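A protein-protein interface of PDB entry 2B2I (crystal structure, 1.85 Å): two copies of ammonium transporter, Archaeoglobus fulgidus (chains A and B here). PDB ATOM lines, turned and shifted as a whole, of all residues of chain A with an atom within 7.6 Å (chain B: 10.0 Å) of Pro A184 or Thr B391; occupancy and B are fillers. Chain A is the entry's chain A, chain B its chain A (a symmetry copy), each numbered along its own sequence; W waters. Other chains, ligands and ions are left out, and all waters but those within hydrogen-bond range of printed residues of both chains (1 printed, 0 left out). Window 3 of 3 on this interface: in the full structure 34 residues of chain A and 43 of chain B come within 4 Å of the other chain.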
ATOM      1  N   TYR A  27      16.027 -10.962   2.266  1.00  0.00           N
ATOM      2  CA  TYR A  27      17.347 -11.584   2.126  1.00  0.00           C
ATOM      3  C   TYR A  27      17.322 -12.910   1.355  1.00  0.00           C
ATOM      4  O   TYR A  27      18.177 -13.154   0.494  1.00  0.00           O
ATOM      5  CB  TYR A  27      17.988 -11.831   3.500  1.00  0.00           C
ATOM      6  CG  TYR A  27      18.455 -10.586   4.240  1.00  0.00           C
ATOM      7  CD1 TYR A  27      18.728  -9.395   3.558  1.00  0.00           C
ATOM      8  CD2 TYR A  27      18.675 -10.619   5.622  1.00  0.00           C
ATOM      9  CE1 TYR A  27      19.214  -8.275   4.235  1.00  0.00           C
ATOM     10  CE2 TYR A  27      19.159  -9.503   6.307  1.00  0.00           C
ATOM     11  CZ  TYR A  27      19.425  -8.341   5.608  1.00  0.00           C
ATOM     12  OH  TYR A  27      19.910  -7.246   6.281  1.00  0.00           O
ATOM     13  N   ALA A  28      16.346 -13.762   1.664  1.00  0.00           N
ATOM     14  CA  ALA A  28      16.232 -15.075   1.024  1.00  0.00           C
ATOM     15  C   ALA A  28      16.260 -15.036  -0.503  1.00  0.00           C
ATOM     16  O   ALA A  28      16.891 -15.884  -1.149  1.00  0.00           O
ATOM     17  CB  ALA A  28      14.963 -15.771   1.497  1.00  0.00           C
ATOM     18  N   GLY A  29      15.582 -14.054  -1.082  1.00  0.00           N
ATOM     19  CA  GLY A  29      15.546 -13.958  -2.526  1.00  0.00           C
ATOM     20  C   GLY A  29      16.885 -13.664  -3.160  1.00  0.00           C
ATOM     21  O   GLY A  29      17.102 -13.985  -4.322  1.00  0.00           O
ATOM     22  N   MET A  30      17.794 -13.060  -2.399  1.00  0.00           N
ATOM     23  CA  MET A  30      19.106 -12.716  -2.935  1.00  0.00           C
ATOM     24  C   MET A  30      20.156 -13.808  -2.770  1.00  0.00           C
ATOM     25  O   MET A  30      21.268 -13.673  -3.286  1.00  0.00           O
ATOM     26  CB  MET A  30      19.619 -11.415  -2.302  1.00  0.00           C
ATOM     27  CG  MET A  30      18.704 -10.214  -2.509  1.00  0.00           C
ATOM     28  SD  MET A  30      19.300  -8.698  -1.712  1.00  0.00           S
ATOM     29  CE  MET A  30      19.035  -9.098  -0.015  1.00  0.00           C
ATOM     30  N   VAL A  31      19.836 -14.877  -2.043  1.00  0.00           N
ATOM     31  CA  VAL A  31      20.801 -15.964  -1.897  1.00  0.00           C
ATOM     32  C   VAL A  31      20.447 -17.086  -2.867  1.00  0.00           C
ATOM     33  O   VAL A  31      19.443 -17.021  -3.587  1.00  0.00           O
ATOM     34  CB  VAL A  31      20.863 -16.535  -0.433  1.00  0.00           C
ATOM     35  CG1 VAL A  31      21.212 -15.420   0.553  1.00  0.00           C
ATOM     36  CG2 VAL A  31      19.559 -17.215  -0.046  1.00  0.00           C
ATOM     37  N   ARG A  32      21.284 -18.113  -2.894  1.00  0.00           N
ATOM     38  CA  ARG A  32      21.062 -19.241  -3.777  1.00  0.00           C
ATOM     39  C   ARG A  32      19.950 -20.134  -3.287  1.00  0.00           C
ATOM     40  O   ARG A  32      19.674 -20.225  -2.088  1.00  0.00           O
ATOM     41  CB  ARG A  32      22.342 -20.049  -3.928  1.00  0.00           C
ATOM     42  CG  ARG A  32      23.326 -19.418  -4.889  1.00  0.00           C
ATOM     43  CD  ARG A  32      24.729 -19.955  -4.670  1.00  0.00           C
ATOM     44  NE  ARG A  32      25.310 -19.506  -3.406  1.00  0.00           N
ATOM     45  CZ  ARG A  32      26.583 -19.698  -3.066  1.00  0.00           C
ATOM     46  NH1 ARG A  32      27.401 -20.333  -3.896  1.00  0.00           N
ATOM     47  NH2 ARG A  32      27.048 -19.245  -1.910  1.00  0.00           N
ATOM     48  N   ARG A  33      19.322 -20.807  -4.236  1.00  0.00           N
ATOM     49  CA  ARG A  33      18.212 -21.690  -3.957  1.00  0.00           C
ATOM     50  C   ARG A  33      18.515 -22.659  -2.827  1.00  0.00           C
ATOM     51  O   ARG A  33      17.644 -22.946  -2.005  1.00  0.00           O
ATOM     52  CB  ARG A  33      17.856 -22.443  -5.232  1.00  0.00           C
ATOM     53  CG  ARG A  33      16.540 -23.160  -5.166  1.00  0.00           C
ATOM     54  CD  ARG A  33      16.246 -23.818  -6.495  1.00  0.00           C
ATOM     55  NE  ARG A  33      15.453 -25.026  -6.312  1.00  0.00           N
ATOM     56  CZ  ARG A  33      15.158 -25.878  -7.286  1.00  0.00           C
ATOM     57  NH1 ARG A  33      15.588 -25.650  -8.520  1.00  0.00           N
ATOM     58  NH2 ARG A  33      14.449 -26.969  -7.021  1.00  0.00           N
ATOM     59  N   LYS A  34      19.751 -23.152  -2.768  1.00  0.00           N
ATOM     60  CA  LYS A  34      20.138 -24.114  -1.722  1.00  0.00           C
ATOM     61  C   LYS A  34      20.212 -23.526  -0.311  1.00  0.00           C
ATOM     62  O   LYS A  34      20.414 -24.271   0.654  1.00  0.00           O
ATOM     63  CB  LYS A  34      21.491 -24.746  -2.050  1.00  0.00           C
ATOM     64  CG  LYS A  34      22.653 -23.768  -2.035  1.00  0.00           C
ATOM     65  CD  LYS A  34      23.954 -24.481  -2.352  1.00  0.00           C
ATOM     66  CE  LYS A  34      25.097 -23.503  -2.511  1.00  0.00           C
ATOM     67  NZ  LYS A  34      26.324 -24.195  -3.016  1.00  0.00           N
ATOM     68  N   TYR A 180      33.268 -15.717  -9.039  1.00  0.00           N
ATOM     69  CA  TYR A 180      32.034 -15.430  -9.752  1.00  0.00           C
ATOM     70  C   TYR A 180      30.982 -14.798  -8.843  1.00  0.00           C
ATOM     71  O   TYR A 180      30.944 -15.055  -7.636  1.00  0.00           O
ATOM     72  CB  TYR A 180      31.498 -16.727 -10.363  1.00  0.00           C
ATOM     73  CG  TYR A 180      30.134 -16.619 -11.010  1.00  0.00           C
ATOM     74  CD1 TYR A 180      29.947 -15.897 -12.197  1.00  0.00           C
ATOM     75  CD2 TYR A 180      29.027 -17.242 -10.435  1.00  0.00           C
ATOM     76  CE1 TYR A 180      28.682 -15.803 -12.793  1.00  0.00           C
ATOM     77  CE2 TYR A 180      27.762 -17.152 -11.017  1.00  0.00           C
ATOM     78  CZ  TYR A 180      27.593 -16.435 -12.192  1.00  0.00           C
ATOM     79  OH  TYR A 180      26.337 -16.357 -12.761  1.00  0.00           O
ATOM     80  N   SER A 181      30.134 -13.964  -9.435  1.00  0.00           N
ATOM     81  CA  SER A 181      29.075 -13.292  -8.699  1.00  0.00           C
ATOM     82  C   SER A 181      27.997 -14.294  -8.287  1.00  0.00           C
ATOM     83  O   SER A 181      27.704 -15.239  -9.016  1.00  0.00           O
ATOM     84  CB  SER A 181      28.462 -12.192  -9.569  1.00  0.00           C
ATOM     85  OG  SER A 181      27.440 -11.499  -8.870  1.00  0.00           O
ATOM     86  N   ILE A 182      27.422 -14.090  -7.107  1.00  0.00           N
ATOM     87  CA  ILE A 182      26.368 -14.964  -6.600  1.00  0.00           C
ATOM     88  C   ILE A 182      25.029 -14.391  -7.038  1.00  0.00           C
ATOM     89  O   ILE A 182      24.649 -13.311  -6.593  1.00  0.00           O
ATOM     90  CB  ILE A 182      26.376 -15.011  -5.059  1.00  0.00           C
ATOM     91  CG1 ILE A 182      27.734 -15.502  -4.555  1.00  0.00           C
ATOM     92  CG2 ILE A 182      25.227 -15.873  -4.557  1.00  0.00           C
ATOM     93  CD1 ILE A 182      28.112 -16.872  -5.035  1.00  0.00           C
ATOM     94  N   GLU A 183      24.304 -15.102  -7.895  1.00  0.00           N
ATOM     95  CA  GLU A 183      23.017 -14.592  -8.364  1.00  0.00           C
ATOM     96  C   GLU A 183      21.826 -14.861  -7.423  1.00  0.00           C
ATOM     97  O   GLU A 183      21.746 -15.891  -6.763  1.00  0.00           O
ATOM     98  CB  GLU A 183      22.700 -15.159  -9.755  1.00  0.00           C
ATOM     99  CG  GLU A 183      23.783 -14.951 -10.822  1.00  0.00           C
ATOM    100  CD  GLU A 183      24.219 -13.505 -10.962  1.00  0.00           C
ATOM    101  OE1 GLU A 183      23.345 -12.609 -10.954  1.00  0.00           O
ATOM    102  OE2 GLU A 183      25.443 -13.260 -11.091  1.00  0.00           O
ATOM    103  N   PRO A 184      20.887 -13.915  -7.341  1.00  0.00           N
ATOM    104  CA  PRO A 184      19.738 -14.143  -6.461  1.00  0.00           C
ATOM    105  C   PRO A 184      18.832 -15.213  -7.078  1.00  0.00           C
ATOM    106  O   PRO A 184      18.544 -15.165  -8.272  1.00  0.00           O
ATOM    107  CB  PRO A 184      19.070 -12.775  -6.415  1.00  0.00           C
ATOM    108  CG  PRO A 184      19.388 -12.196  -7.775  1.00  0.00           C
ATOM    109  CD  PRO A 184      20.850 -12.571  -7.940  1.00  0.00           C
ATOM    110  N   HIS A 185      18.377 -16.176  -6.287  1.00  0.00           N
ATOM    111  CA  HIS A 185      17.528 -17.215  -6.851  1.00  0.00           C
ATOM    112  C   HIS A 185      16.096 -16.734  -7.126  1.00  0.00           C
ATOM    113  O   HIS A 185      15.426 -17.254  -8.020  1.00  0.00           O
ATOM    114  CB  HIS A 185      17.499 -18.454  -5.943  1.00  0.00           C
ATOM    115  CG  HIS A 185      16.472 -18.390  -4.858  1.00  0.00           C
ATOM    116  ND1 HIS A 185      16.657 -17.670  -3.699  1.00  0.00           N
ATOM    117  CD2 HIS A 185      15.227 -18.918  -4.781  1.00  0.00           C
ATOM    118  CE1 HIS A 185      15.567 -17.753  -2.954  1.00  0.00           C
ATOM    119  NE2 HIS A 185      14.684 -18.504  -3.588  1.00  0.00           N
ATOM    120  N   SER A 186      15.619 -15.741  -6.379  1.00  0.00           N
ATOM    121  CA  SER A 186      14.255 -15.265  -6.601  1.00  0.00           C
ATOM    122  C   SER A 186      14.089 -13.796  -6.282  1.00  0.00           C
ATOM    123  O   SER A 186      13.824 -13.419  -5.141  1.00  0.00           O
ATOM    124  CB  SER A 186      13.268 -16.067  -5.757  1.00  0.00           C
ATOM    125  OG  SER A 186      11.950 -15.597  -5.981  1.00  0.00           O
ATOM    126  N   ILE A 187      14.241 -12.958  -7.292  1.00  0.00           N
ATOM    127  CA  ILE A 187      14.090 -11.534  -7.057  1.00  0.00           C
ATOM    128  C   ILE A 187      12.667 -11.245  -6.573  1.00  0.00           C
ATOM    129  O   ILE A 187      12.472 -10.421  -5.681  1.00  0.00           O
ATOM    130  CB  ILE A 187      14.469 -10.738  -8.324  1.00  0.00           C
ATOM    131  CG1 ILE A 187      15.992 -10.824  -8.515  1.00  0.00           C
ATOM    132  CG2 ILE A 187      14.042  -9.282  -8.197  1.00  0.00           C
ATOM    133  CD1 ILE A 187      16.519 -10.130  -9.753  1.00  0.00           C
ATOM    134  N   PRO A 188      11.653 -11.934  -7.139  1.00  0.00           N
ATOM    135  CA  PRO A 188      10.283 -11.689  -6.685  1.00  0.00           C
ATOM    136  C   PRO A 188      10.122 -11.950  -5.187  1.00  0.00           C
ATOM    137  O   PRO A 188       9.382 -11.242  -4.510  1.00  0.00           O
ATOM    138  CB  PRO A 188       9.460 -12.654  -7.535  1.00  0.00           C
ATOM    139  CG  PRO A 188      10.195 -12.628  -8.831  1.00  0.00           C
ATOM    140  CD  PRO A 188      11.650 -12.721  -8.390  1.00  0.00           C
ATOM    141  N   THR A 190      12.394 -11.536  -2.968  1.00  0.00           N
ATOM    142  CA  THR A 190      12.995 -10.377  -2.340  1.00  0.00           C
ATOM    143  C   THR A 190      12.039  -9.173  -2.387  1.00  0.00           C
ATOM    144  O   THR A 190      11.891  -8.452  -1.389  1.00  0.00           O
ATOM    145  CB  THR A 190      14.326 -10.034  -3.017  1.00  0.00           C
ATOM    146  OG1 THR A 190      15.317 -10.963  -2.568  1.00  0.00           O
ATOM    147  CG2 THR A 190      14.772  -8.620  -2.673  1.00  0.00           C
ATOM    148  N   LEU A 247      16.395  -4.463  -7.663  1.00  0.00           N
ATOM    149  CA  LEU A 247      17.142  -4.584  -6.409  1.00  0.00           C
ATOM    150  C   LEU A 247      17.713  -3.253  -5.959  1.00  0.00           C
ATOM    151  O   LEU A 247      17.607  -2.897  -4.786  1.00  0.00           O
ATOM    152  CB  LEU A 247      18.282  -5.604  -6.556  1.00  0.00           C
ATOM    153  CG  LEU A 247      17.835  -7.031  -6.894  1.00  0.00           C
ATOM    154  CD1 LEU A 247      19.041  -7.953  -6.977  1.00  0.00           C
ATOM    155  CD2 LEU A 247      16.857  -7.521  -5.841  1.00  0.00           C
ATOM    156  N   TYR A 390      12.645 -25.880  -2.798  1.00  0.00           N
ATOM    157  CA  TYR A 390      11.657 -26.157  -3.831  1.00  0.00           C
ATOM    158  C   TYR A 390      11.818 -27.476  -4.547  1.00  0.00           C
ATOM    159  O   TYR A 390      12.919 -28.004  -4.707  1.00  0.00           O
ATOM    160  CB  TYR A 390      11.668 -25.079  -4.908  1.00  0.00           C
ATOM    161  CG  TYR A 390      11.824 -23.683  -4.396  1.00  0.00           C
ATOM    162  CD1 TYR A 390      13.091 -23.136  -4.209  1.00  0.00           C
ATOM    163  CD2 TYR A 390      10.707 -22.898  -4.106  1.00  0.00           C
ATOM    164  CE1 TYR A 390      13.245 -21.832  -3.748  1.00  0.00           C
ATOM    165  CE2 TYR A 390      10.845 -21.595  -3.645  1.00  0.00           C
ATOM    166  CZ  TYR A 390      12.112 -21.072  -3.470  1.00  0.00           C
ATOM    167  OH  TYR A 390      12.261 -19.790  -3.017  1.00  0.00           O
ATOM    168  N   ARG B  33       7.727 -15.497 -17.128  1.00  0.00           N
ATOM    169  CA  ARG B  33       8.859 -15.474 -16.229  1.00  0.00           C
ATOM    170  C   ARG B  33       9.870 -14.402 -16.603  1.00  0.00           C
ATOM    171  O   ARG B  33      10.440 -13.753 -15.726  1.00  0.00           O
ATOM    172  CB  ARG B  33       9.509 -16.851 -16.227  1.00  0.00           C
ATOM    173  CG  ARG B  33      10.499 -17.053 -15.120  1.00  0.00           C
ATOM    174  CD  ARG B  33      11.038 -18.465 -15.162  1.00  0.00           C
ATOM    175  NE  ARG B  33      12.403 -18.516 -14.657  1.00  0.00           N
ATOM    176  CZ  ARG B  33      13.172 -19.597 -14.699  1.00  0.00           C
ATOM    177  NH1 ARG B  33      12.705 -20.725 -15.219  1.00  0.00           N
ATOM    178  NH2 ARG B  33      14.416 -19.543 -14.238  1.00  0.00           N
ATOM    179  N   VAL B  37      10.022  -9.581 -12.972  1.00  0.00           N
ATOM    180  CA  VAL B  37      10.637  -8.459 -12.258  1.00  0.00           C
ATOM    181  C   VAL B  37      10.094  -7.109 -12.751  1.00  0.00           C
ATOM    182  O   VAL B  37       9.776  -6.228 -11.951  1.00  0.00           O
ATOM    183  CB  VAL B  37      12.174  -8.463 -12.429  1.00  0.00           C
ATOM    184  CG1 VAL B  37      12.778  -7.150 -11.906  1.00  0.00           C
ATOM    185  CG2 VAL B  37      12.777  -9.639 -11.681  1.00  0.00           C
ATOM    186  N   ASP B 381      12.855  -8.046 -18.113  1.00  0.00           N
ATOM    187  CA  ASP B 381      13.667  -8.180 -16.910  1.00  0.00           C
ATOM    188  C   ASP B 381      15.122  -7.931 -17.289  1.00  0.00           C
ATOM    189  O   ASP B 381      15.809  -7.117 -16.681  1.00  0.00           O
ATOM    190  CB  ASP B 381      13.513  -9.578 -16.321  1.00  0.00           C
ATOM    191  CG  ASP B 381      12.157  -9.777 -15.699  1.00  0.00           C
ATOM    192  OD1 ASP B 381      11.318  -8.861 -15.859  1.00  0.00           O
ATOM    193  OD2 ASP B 381      11.931 -10.825 -15.055  1.00  0.00           O
ATOM    194  N   LEU B 382      15.576  -8.640 -18.314  1.00  0.00           N
ATOM    195  CA  LEU B 382      16.940  -8.504 -18.800  1.00  0.00           C
ATOM    196  C   LEU B 382      17.163  -7.179 -19.507  1.00  0.00           C
ATOM    197  O   LEU B 382      18.084  -6.430 -19.185  1.00  0.00           O
ATOM    198  CB  LEU B 382      17.265  -9.610 -19.804  1.00  0.00           C
ATOM    199  CG  LEU B 382      18.313 -10.681 -19.490  1.00  0.00           C
ATOM    200  CD1 LEU B 382      19.380 -10.146 -18.535  1.00  0.00           C
ATOM    201  CD2 LEU B 382      17.604 -11.880 -18.891  1.00  0.00           C
ATOM    202  N   GLU B 386      18.086  -5.527 -16.582  1.00  0.00           N
ATOM    203  CA  GLU B 386      19.304  -6.321 -16.570  1.00  0.00           C
ATOM    204  C   GLU B 386      19.291  -7.272 -15.376  1.00  0.00           C
ATOM    205  O   GLU B 386      20.304  -7.463 -14.706  1.00  0.00           O
ATOM    206  CB  GLU B 386      20.533  -5.413 -16.528  1.00  0.00           C
ATOM    207  CG  GLU B 386      20.700  -4.630 -17.809  1.00  0.00           C
ATOM    208  CD  GLU B 386      22.062  -3.967 -17.945  1.00  0.00           C
ATOM    209  OE1 GLU B 386      22.289  -3.326 -18.994  1.00  0.00           O
ATOM    210  OE2 GLU B 386      22.899  -4.088 -17.021  1.00  0.00           O
ATOM    211  N   GLU B 387      18.129  -7.863 -15.115  1.00  0.00           N
ATOM    212  CA  GLU B 387      17.987  -8.817 -14.029  1.00  0.00           C
ATOM    213  C   GLU B 387      17.300 -10.075 -14.544  1.00  0.00           C
ATOM    214  O   GLU B 387      16.744 -10.083 -15.640  1.00  0.00           O
ATOM    215  CB  GLU B 387      17.161  -8.211 -12.894  1.00  0.00           C
ATOM    216  CG  GLU B 387      17.920  -7.202 -12.066  1.00  0.00           C
ATOM    217  CD  GLU B 387      17.065  -6.532 -11.005  1.00  0.00           C
ATOM    218  OE1 GLU B 387      17.636  -6.085  -9.993  1.00  0.00           O
ATOM    219  OE2 GLU B 387      15.833  -6.430 -11.176  1.00  0.00           O
ATOM    220  N   VAL B 388      17.359 -11.139 -13.750  1.00  0.00           N
ATOM    221  CA  VAL B 388      16.707 -12.403 -14.075  1.00  0.00           C
ATOM    222  C   VAL B 388      15.881 -12.747 -12.841  1.00  0.00           C
ATOM    223  O   VAL B 388      16.417 -12.838 -11.733  1.00  0.00           O
ATOM    224  CB  VAL B 388      17.734 -13.529 -14.347  1.00  0.00           C
ATOM    225  CG1 VAL B 388      17.009 -14.844 -14.630  1.00  0.00           C
ATOM    226  CG2 VAL B 388      18.610 -13.149 -15.531  1.00  0.00           C
ATOM    227  N   ALA B 389      14.579 -12.922 -13.033  1.00  0.00           N
ATOM    228  CA  ALA B 389      13.670 -13.218 -11.929  1.00  0.00           C
ATOM    229  C   ALA B 389      14.065 -14.416 -11.071  1.00  0.00           C
ATOM    230  O   ALA B 389      14.175 -14.301  -9.857  1.00  0.00           O
ATOM    231  CB  ALA B 389      12.254 -13.414 -12.470  1.00  0.00           C
ATOM    232  N   TYR B 390      14.278 -15.567 -11.700  1.00  0.00           N
ATOM    233  CA  TYR B 390      14.635 -16.760 -10.946  1.00  0.00           C
ATOM    234  C   TYR B 390      15.788 -17.559 -11.503  1.00  0.00           C
ATOM    235  O   TYR B 390      16.039 -17.596 -12.709  1.00  0.00           O
ATOM    236  CB  TYR B 390      13.457 -17.722 -10.842  1.00  0.00           C
ATOM    237  CG  TYR B 390      12.135 -17.067 -10.599  1.00  0.00           C
ATOM    238  CD1 TYR B 390      11.350 -16.639 -11.667  1.00  0.00           C
ATOM    239  CD2 TYR B 390      11.655 -16.883  -9.302  1.00  0.00           C
ATOM    240  CE1 TYR B 390      10.112 -16.044 -11.450  1.00  0.00           C
ATOM    241  CE2 TYR B 390      10.422 -16.290  -9.069  1.00  0.00           C
ATOM    242  CZ  TYR B 390       9.660 -15.875 -10.144  1.00  0.00           C
ATOM    243  OH  TYR B 390       8.442 -15.291  -9.928  1.00  0.00           O
ATOM    244  N   THR B 391      16.457 -18.231 -10.582  1.00  0.00           N
ATOM    245  CA  THR B 391      17.566 -19.104 -10.886  1.00  0.00           C
ATOM    246  C   THR B 391      17.317 -20.357 -10.058  1.00  0.00           C
ATOM    247  O   THR B 391      17.785 -20.373  -8.895  1.00  0.00           O
ATOM    248  CB  THR B 391      18.896 -18.471 -10.463  1.00  0.00           C
ATOM    249  OG1 THR B 391      19.113 -17.268 -11.219  1.00  0.00           O
ATOM    250  CG2 THR B 391      20.048 -19.445 -10.706  1.00  0.00           C
HETATM  251  O   HOH W   1      19.980 -20.561  -7.075  1.00  0.00           O
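A ring nitrogen (NE2) of His A185 lies within hydrogen-bond range of the side-chain hydroxyl of Tyr A390. The backbone NH (N) of Leu B382 lies within hydrogen-bond range of the backbone carbonyl oxygen (O) of Glu B387 (3.3 Å). The backbone carbonyl oxygen (O) of Asp B381 is in hydrogen-bond range of the backbone NH (N) of Glu B387, 2.9 Å away. N of His A185 is in hydrogen-bond range of O of Gly A29 (3.2 Å). The backbone carbonyl oxygen (O) of Ala A28 sits close to a ring nitrogen (ND1) of His A185 (3.1 Å). The backbone NH of Val B37 lies within hydrogen-bond range of the side-chain carboxylate of Asp B381 (3.1 Å).
No residue of chain B comes within 4 Å of Glu A183. Pro A184 touches one residue of chain B. Of the printed residues of chain B, His A185 touches Ala B389, Tyr B390 and Thr B391. Printed residues of chain B within 4 Å of Pro A188: Ala B389 and Tyr B390. Of the printed residues of chain A, Glu B387 touches Ile A187 (3.7 Å) and Leu A247 (3.1 Å). Of the printed residues of chain A, Val B388 touches Ile A187. Of the printed residues of chain A, Tyr B390 touches His A185, Ser A186 and Pro A188. Thr B391 touches two residues of chain A. The nearest residue of chain A that does not touch Thr B391 is Arg A33 (4.2 Å).
Water W1 bridges the backbone carbonyl oxygen (O) of Thr B391 (2.9 Å) and the backbone NH (N) of Arg A33 (2.9 Å).
Hydrophobic or aromatic side chains of chain B within 4 Å of the printed part of chain A: Val B37 and Tyr B390. Of the 20 printed residues of chain A, 6 touch a printed residue of chain B. Hydrophobic or aromatic side chains of chain A within 4 Å of the printed part of chain B: His A185, Ile A187, Pro A188 and Leu A247. Among the printed residues, 13 pairs touch across the chains.
Thr B391 touches Pro A184. O of Ala B389 touches O of His A185 (3.7 Å). O of His A185 touches CA of Tyr B390, at 3.1 Å. Ser A186 touches Ala B389. Tyr B390 touches Ser A186. Val B37 touches Ile A187. CD1 of Ile A187 touches CB of Glu B387, 3.7 Å away. Val B388 touches Ile A187. O of Ala B389 touches CD of Pro A188, at 3.3 Å. OH of Tyr B390 touches CG of Pro A188 (3.4 Å).
Positions printed for both chains: 33 and 390.
The backbone NH of Thr B391 lies within hydrogen-bond range of the backbone carbonyl oxygen of His A185. The backbone NH (N) of Leu A247 sits at hydrogen-bond distance from the side-chain carboxylate (OE1) of Glu B387 (3.1 Å). The backbone NH (N) of Ile A187 sits at hydrogen-bond distance from the backbone carbonyl oxygen (O) of Ala B389 (2.9 Å).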
